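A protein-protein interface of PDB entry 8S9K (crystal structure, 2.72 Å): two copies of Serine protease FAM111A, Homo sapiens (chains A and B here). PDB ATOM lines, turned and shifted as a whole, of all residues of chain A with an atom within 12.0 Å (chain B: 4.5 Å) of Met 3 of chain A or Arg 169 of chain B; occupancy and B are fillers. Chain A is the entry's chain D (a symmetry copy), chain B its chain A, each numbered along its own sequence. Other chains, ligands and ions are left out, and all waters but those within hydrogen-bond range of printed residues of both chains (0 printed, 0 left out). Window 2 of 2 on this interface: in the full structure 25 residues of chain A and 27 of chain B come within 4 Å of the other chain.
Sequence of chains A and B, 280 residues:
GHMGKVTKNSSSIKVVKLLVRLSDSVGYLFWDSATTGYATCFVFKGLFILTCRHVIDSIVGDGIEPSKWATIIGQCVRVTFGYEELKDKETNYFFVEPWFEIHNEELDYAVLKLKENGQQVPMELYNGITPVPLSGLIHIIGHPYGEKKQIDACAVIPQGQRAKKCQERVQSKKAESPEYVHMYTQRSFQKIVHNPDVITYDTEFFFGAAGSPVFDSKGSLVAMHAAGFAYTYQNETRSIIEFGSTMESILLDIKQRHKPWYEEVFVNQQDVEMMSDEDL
NH2 of Arg 169 of chain B is in salt-bridge range of OD2 of Asp 202 of chain B, at 2.5 Å. The backbone carbonyl oxygen of Ile 240 of chain B is in hydrogen-bond range of the guanidinium group of Arg 169 of chain B (2.5 Å).
Printed residues of chain B within 4 Å of His 2 of chain A: Arg 169, Asp 202, Tyr 231 and Ile 240. Of chain B, only Arg 169 comes within 4 Å of Met 3 of chain A. Lys 5 of chain A touches none of the printed residues of chain B. Val 6 of chain A touches none of the printed residues of chain B. No residue of chain A comes within 4 Å of Lys 165 of chain B. Cys 166 of chain B touches none of the printed residues of chain A. No residue of chain A comes within 4 Å of Glu 168 of chain B. Arg 169 of chain B touches just these residues of chain A: His 2 and Met 3. No residue of chain A comes within 4 Å of Ser 172 of chain B. Of the printed residues of chain A, Tyr 231 of chain B touches His 2 (3.5 Å). Ile 240 of chain B touches just one residue of chain A: His 2 (3.1 Å). The nearest residue of chain B that does not touch Met 3 of chain A is Tyr 231 of chain B (4.1 Å). The nearest printed residue of chain B that does not touch His 2 of chain A is Ile 157 of chain B (6.2 Å).
Of the 12 printed residues of chain B, 4 touch a printed residue of chain A. Hydrophobic or aromatic side chains of chain B within 4 Å of the printed part of chain A: Tyr 231. Of the 9 printed residues of chain A, 2 touch a printed residue of chain B. Printed residues of chain A that touch a printed residue of chain B: His 2 and Met 3. Hydrophobic or aromatic side chains of chain A that line the printed part of chain B: His 2 and Met 3. Along chain A the printed residues that touch a printed residue of chain B span positions 2 to 3.
Among the printed residues, merely in contact across the chains: His 2 of chain A with Ile 240 of chain B (3.1 Å), His 2 of chain A with Arg 169 of chain B (3.2 Å), Met 3 of chain A with Arg 169 of chain B (3.4 Å) and His 2 of chain A with Tyr 231 of chain B (3.5 Å).
No position is printed for both chains. Of the 5 pairs that touch across the chains among the printed residues, none has its exchanged pair printed and touching as well.
A ring nitrogen (NE2) of His 2 of chain A lies close to the side-chain carboxylate (OD1) of Asp 202 of chain B, at 3.5 Å.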
ATOM      1  N   GLY A   1      14.794 -13.214 -21.153  1.00  0.00           N
ATOM      2  CA  GLY A   1      14.209 -14.091 -22.152  1.00  0.00           C
ATOM      3  C   GLY A   1      14.569 -13.671 -23.562  1.00  0.00           C
ATOM      4  O   GLY A   1      14.083 -12.655 -24.056  1.00  0.00           O
ATOM      5  N   HIS A   2      15.418 -14.460 -24.216  1.00  0.00           N
ATOM      6  CA  HIS A   2      15.987 -14.101 -25.511  1.00  0.00           C
ATOM      7  C   HIS A   2      15.729 -15.165 -26.573  1.00  0.00           C
ATOM      8  O   HIS A   2      16.541 -15.346 -27.483  1.00  0.00           O
ATOM      9  CB  HIS A   2      17.487 -13.837 -25.372  1.00  0.00           C
ATOM     10  CG  HIS A   2      18.206 -14.856 -24.542  1.00  0.00           C
ATOM     11  ND1 HIS A   2      17.742 -16.142 -24.371  1.00  0.00           N
ATOM     12  CD2 HIS A   2      19.354 -14.772 -23.826  1.00  0.00           C
ATOM     13  CE1 HIS A   2      18.573 -16.810 -23.591  1.00  0.00           C
ATOM     14  NE2 HIS A   2      19.559 -16.002 -23.247  1.00  0.00           N
ATOM     15  N   MET A   3      14.601 -15.867 -26.485  1.00  0.00           N
ATOM     16  CA  MET A   3      14.301 -16.929 -27.439  1.00  0.00           C
ATOM     17  C   MET A   3      13.311 -16.525 -28.520  1.00  0.00           C
ATOM     18  O   MET A   3      13.407 -17.027 -29.644  1.00  0.00           O
ATOM     19  CB  MET A   3      13.776 -18.170 -26.711  1.00  0.00           C
ATOM     20  CG  MET A   3      14.882 -19.119 -26.305  1.00  0.00           C
ATOM     21  SD  MET A   3      16.075 -19.304 -27.647  1.00  0.00           S
ATOM     22  CE  MET A   3      15.105 -20.218 -28.845  1.00  0.00           C
ATOM     23  N   GLY A   4      12.366 -15.641 -28.220  1.00  0.00           N
ATOM     24  CA  GLY A   4      11.416 -15.201 -29.222  1.00  0.00           C
ATOM     25  C   GLY A   4      11.491 -13.712 -29.483  1.00  0.00           C
ATOM     26  O   GLY A   4      12.556 -13.104 -29.336  1.00  0.00           O
ATOM     27  N   LYS A   5      10.371 -13.111 -29.878  1.00  0.00           N
ATOM     28  CA  LYS A   5      10.286 -11.663 -30.038  1.00  0.00           C
ATOM     29  C   LYS A   5       9.992 -11.047 -28.674  1.00  0.00           C
ATOM     30  O   LYS A   5       8.880 -11.183 -28.152  1.00  0.00           O
ATOM     31  CB  LYS A   5       9.211 -11.298 -31.057  1.00  0.00           C
ATOM     32  N   VAL A   6      10.983 -10.375 -28.091  1.00  0.00           N
ATOM     33  CA  VAL A   6      10.919  -9.917 -26.709  1.00  0.00           C
ATOM     34  C   VAL A   6      11.351  -8.457 -26.635  1.00  0.00           C
ATOM     35  O   VAL A   6      12.283  -8.038 -27.328  1.00  0.00           O
ATOM     36  CB  VAL A   6      11.798 -10.791 -25.787  1.00  0.00           C
ATOM     37  CG1 VAL A   6      11.781 -10.268 -24.358  1.00  0.00           C
ATOM     38  CG2 VAL A   6      11.339 -12.241 -25.823  1.00  0.00           C
ATOM     39  N   THR A   7      10.663  -7.685 -25.795  1.00  0.00           N
ATOM     40  CA  THR A   7      11.060  -6.324 -25.472  1.00  0.00           C
ATOM     41  C   THR A   7      12.041  -6.340 -24.303  1.00  0.00           C
ATOM     42  O   THR A   7      11.965  -7.197 -23.419  1.00  0.00           O
ATOM     43  CB  THR A   7       9.836  -5.469 -25.121  1.00  0.00           C
ATOM     44  OG1 THR A   7       8.818  -5.657 -26.112  1.00  0.00           O
ATOM     45  CG2 THR A   7      10.202  -3.989 -25.064  1.00  0.00           C
ATOM     46  N   LYS A   8      12.970  -5.387 -24.311  1.00  0.00           N
ATOM     47  CA  LYS A   8      13.999  -5.334 -23.280  1.00  0.00           C
ATOM     48  C   LYS A   8      13.370  -5.037 -21.922  1.00  0.00           C
ATOM     49  O   LYS A   8      12.686  -4.022 -21.751  1.00  0.00           O
ATOM     50  CB  LYS A   8      15.050  -4.280 -23.627  1.00  0.00           C
ATOM     51  CG  LYS A   8      16.467  -4.835 -23.692  1.00  0.00           C
ATOM     52  CD  LYS A   8      17.508  -3.736 -23.838  1.00  0.00           C
ATOM     53  CE  LYS A   8      18.916  -4.314 -23.822  1.00  0.00           C
ATOM     54  NZ  LYS A   8      19.966  -3.258 -23.878  1.00  0.00           N
ATOM     55  N   ASN A   9      13.600  -5.932 -20.960  1.00  0.00           N
ATOM     56  CA  ASN A   9      13.105  -5.769 -19.600  1.00  0.00           C
ATOM     57  C   ASN A   9      14.046  -4.954 -18.725  1.00  0.00           C
ATOM     58  O   ASN A   9      13.603  -4.379 -17.724  1.00  0.00           O
ATOM     59  CB  ASN A   9      12.875  -7.149 -18.968  1.00  0.00           C
ATOM     60  CG  ASN A   9      11.872  -7.121 -17.825  1.00  0.00           C
ATOM     61  OD1 ASN A   9      11.985  -6.326 -16.895  1.00  0.00           O
ATOM     62  ND2 ASN A   9      10.881  -8.003 -17.893  1.00  0.00           N
ATOM     63  N   ILE B 157      18.722 -20.727 -14.724  1.00  0.00           N
ATOM     64  CA  ILE B 157      18.522 -22.038 -15.327  1.00  0.00           C
ATOM     65  C   ILE B 157      19.178 -23.066 -14.405  1.00  0.00           C
ATOM     66  O   ILE B 157      20.414 -23.066 -14.284  1.00  0.00           O
ATOM     67  CB  ILE B 157      19.113 -22.104 -16.740  1.00  0.00           C
ATOM     68  CG1 ILE B 157      18.497 -21.014 -17.620  1.00  0.00           C
ATOM     69  CG2 ILE B 157      18.897 -23.478 -17.351  1.00  0.00           C
ATOM     70  CD1 ILE B 157      19.077 -20.948 -19.010  1.00  0.00           C
ATOM     71  N   LYS B 165      17.514 -27.307 -21.928  1.00  0.00           N
ATOM     72  CA  LYS B 165      17.304 -25.987 -22.516  1.00  0.00           C
ATOM     73  C   LYS B 165      18.126 -25.777 -23.783  1.00  0.00           C
ATOM     74  O   LYS B 165      17.576 -25.498 -24.855  1.00  0.00           O
ATOM     75  CB  LYS B 165      17.636 -24.905 -21.482  1.00  0.00           C
ATOM     76  CG  LYS B 165      16.583 -24.720 -20.400  1.00  0.00           C
ATOM     77  CD  LYS B 165      15.313 -24.101 -20.966  1.00  0.00           C
ATOM     78  CE  LYS B 165      14.288 -23.831 -19.873  1.00  0.00           C
ATOM     79  NZ  LYS B 165      13.076 -23.148 -20.408  1.00  0.00           N
ATOM     80  N   CYS B 166      19.450 -25.932 -23.670  1.00  0.00           N
ATOM     81  CA  CYS B 166      20.337 -25.772 -24.818  1.00  0.00           C
ATOM     82  C   CYS B 166      19.820 -26.538 -26.028  1.00  0.00           C
ATOM     83  O   CYS B 166      19.578 -25.956 -27.093  1.00  0.00           O
ATOM     84  CB  CYS B 166      21.752 -26.236 -24.459  1.00  0.00           C
ATOM     85  SG  CYS B 166      22.669 -25.139 -23.352  1.00  0.00           S
ATOM     86  N   GLN B 167      19.608 -27.848 -25.868  1.00  0.00           N
ATOM     87  CA  GLN B 167      19.196 -28.660 -27.008  1.00  0.00           C
ATOM     88  C   GLN B 167      17.852 -28.206 -27.557  1.00  0.00           C
ATOM     89  O   GLN B 167      17.613 -28.300 -28.766  1.00  0.00           O
ATOM     90  CB  GLN B 167      19.143 -30.137 -26.623  1.00  0.00           C
ATOM     91  CG  GLN B 167      19.070 -31.068 -27.825  1.00  0.00           C
ATOM     92  CD  GLN B 167      18.965 -32.527 -27.435  1.00  0.00           C
ATOM     93  OE1 GLN B 167      18.718 -32.856 -26.277  1.00  0.00           O
ATOM     94  NE2 GLN B 167      19.153 -33.413 -28.408  1.00  0.00           N
ATOM     95  N   GLU B 168      16.965 -27.705 -26.693  1.00  0.00           N
ATOM     96  CA  GLU B 168      15.721 -27.125 -27.184  1.00  0.00           C
ATOM     97  C   GLU B 168      16.008 -25.889 -28.024  1.00  0.00           C
ATOM     98  O   GLU B 168      15.526 -25.764 -29.156  1.00  0.00           O
ATOM     99  CB  GLU B 168      14.797 -26.777 -26.014  1.00  0.00           C
ATOM    100  CG  GLU B 168      14.457 -27.941 -25.092  1.00  0.00           C
ATOM    101  CD  GLU B 168      13.420 -27.569 -24.044  1.00  0.00           C
ATOM    102  OE1 GLU B 168      12.241 -27.377 -24.411  1.00  0.00           O
ATOM    103  OE2 GLU B 168      13.786 -27.457 -22.854  1.00  0.00           O
ATOM    104  N   ARG B 169      16.833 -24.981 -27.494  1.00  0.00           N
ATOM    105  CA  ARG B 169      17.045 -23.693 -28.145  1.00  0.00           C
ATOM    106  C   ARG B 169      17.749 -23.844 -29.487  1.00  0.00           C
ATOM    107  O   ARG B 169      17.590 -22.990 -30.368  1.00  0.00           O
ATOM    108  CB  ARG B 169      17.829 -22.772 -27.210  1.00  0.00           C
ATOM    109  CG  ARG B 169      16.972 -22.211 -26.083  1.00  0.00           C
ATOM    110  CD  ARG B 169      17.615 -22.367 -24.720  1.00  0.00           C
ATOM    111  NE  ARG B 169      16.739 -21.870 -23.664  1.00  0.00           N
ATOM    112  CZ  ARG B 169      16.907 -20.711 -23.037  1.00  0.00           C
ATOM    113  NH1 ARG B 169      17.932 -19.930 -23.352  1.00  0.00           N
ATOM    114  NH2 ARG B 169      16.058 -20.335 -22.090  1.00  0.00           N
ATOM    115  N   VAL B 170      18.514 -24.919 -29.669  1.00  0.00           N
ATOM    116  CA  VAL B 170      19.112 -25.185 -30.971  1.00  0.00           C
ATOM    117  C   VAL B 170      18.071 -25.738 -31.938  1.00  0.00           C
ATOM    118  O   VAL B 170      18.069 -25.398 -33.128  1.00  0.00           O
ATOM    119  CB  VAL B 170      20.313 -26.136 -30.815  1.00  0.00           C
ATOM    120  CG1 VAL B 170      20.863 -26.533 -32.174  1.00  0.00           C
ATOM    121  CG2 VAL B 170      21.395 -25.484 -29.969  1.00  0.00           C
ATOM    122  N   GLN B 171      17.159 -26.580 -31.448  1.00  0.00           N
ATOM    123  CA  GLN B 171      16.157 -27.183 -32.319  1.00  0.00           C
ATOM    124  C   GLN B 171      14.972 -26.263 -32.583  1.00  0.00           C
ATOM    125  O   GLN B 171      14.239 -26.485 -33.554  1.00  0.00           O
ATOM    126  CB  GLN B 171      15.660 -28.501 -31.720  1.00  0.00           C
ATOM    127  CG  GLN B 171      16.738 -29.566 -31.595  1.00  0.00           C
ATOM    128  CD  GLN B 171      17.293 -29.994 -32.938  1.00  0.00           C
ATOM    129  OE1 GLN B 171      16.566 -30.066 -33.928  1.00  0.00           O
ATOM    130  NE2 GLN B 171      18.591 -30.276 -32.977  1.00  0.00           N
ATOM    131  N   SER B 172      14.770 -25.246 -31.753  1.00  0.00           N
ATOM    132  CA  SER B 172      13.667 -24.310 -31.939  1.00  0.00           C
ATOM    133  C   SER B 172      13.963 -23.339 -33.077  1.00  0.00           C
ATOM    134  O   SER B 172      13.195 -22.412 -33.333  1.00  0.00           O
ATOM    135  CB  SER B 172      13.393 -23.540 -30.645  1.00  0.00           C
ATOM    136  OG  SER B 172      12.325 -22.624 -30.811  1.00  0.00           O
ATOM    137  N   ASP B 202      19.191 -16.708 -18.120  1.00  0.00           N
ATOM    138  CA  ASP B 202      18.746 -16.006 -19.322  1.00  0.00           C
ATOM    139  C   ASP B 202      18.733 -14.512 -19.030  1.00  0.00           C
ATOM    140  O   ASP B 202      17.921 -14.038 -18.227  1.00  0.00           O
ATOM    141  CB  ASP B 202      17.364 -16.483 -19.764  1.00  0.00           C
ATOM    142  CG  ASP B 202      17.391 -17.869 -20.364  1.00  0.00           C
ATOM    143  OD1 ASP B 202      18.452 -18.269 -20.885  1.00  0.00           O
ATOM    144  OD2 ASP B 202      16.349 -18.556 -20.319  1.00  0.00           O
ATOM    145  N   TYR B 231      24.342 -15.510 -31.493  1.00  0.00           N
ATOM    146  CA  TYR B 231      23.906 -15.889 -32.827  1.00  0.00           C
ATOM    147  C   TYR B 231      23.105 -14.731 -33.406  1.00  0.00           C
ATOM    148  O   TYR B 231      22.749 -13.782 -32.702  1.00  0.00           O
ATOM    149  CB  TYR B 231      23.089 -17.187 -32.814  1.00  0.00           C
ATOM    150  CG  TYR B 231      21.732 -17.091 -32.144  1.00  0.00           C
ATOM    151  CD1 TYR B 231      21.596 -17.269 -30.772  1.00  0.00           C
ATOM    152  CD2 TYR B 231      20.582 -16.846 -32.888  1.00  0.00           C
ATOM    153  CE1 TYR B 231      20.356 -17.192 -30.158  1.00  0.00           C
ATOM    154  CE2 TYR B 231      19.340 -16.767 -32.283  1.00  0.00           C
ATOM    155  CZ  TYR B 231      19.232 -16.942 -30.920  1.00  0.00           C
ATOM    156  OH  TYR B 231      17.997 -16.862 -30.317  1.00  0.00           O
ATOM    157  N   ILE B 240      22.120 -17.833 -26.725  1.00  0.00           N
ATOM    158  CA  ILE B 240      21.427 -19.061 -26.348  1.00  0.00           C
ATOM    159  C   ILE B 240      21.316 -19.178 -24.832  1.00  0.00           C
ATOM    160  O   ILE B 240      20.224 -19.379 -24.288  1.00  0.00           O
ATOM    161  CB  ILE B 240      22.138 -20.283 -26.958  1.00  0.00           C
ATOM    162  CG1 ILE B 240      22.029 -20.248 -28.483  1.00  0.00           C
ATOM    163  CG2 ILE B 240      21.558 -21.576 -26.403  1.00  0.00           C
ATOM    164  CD1 ILE B 240      22.625 -21.455 -29.165  1.00  0.00           C
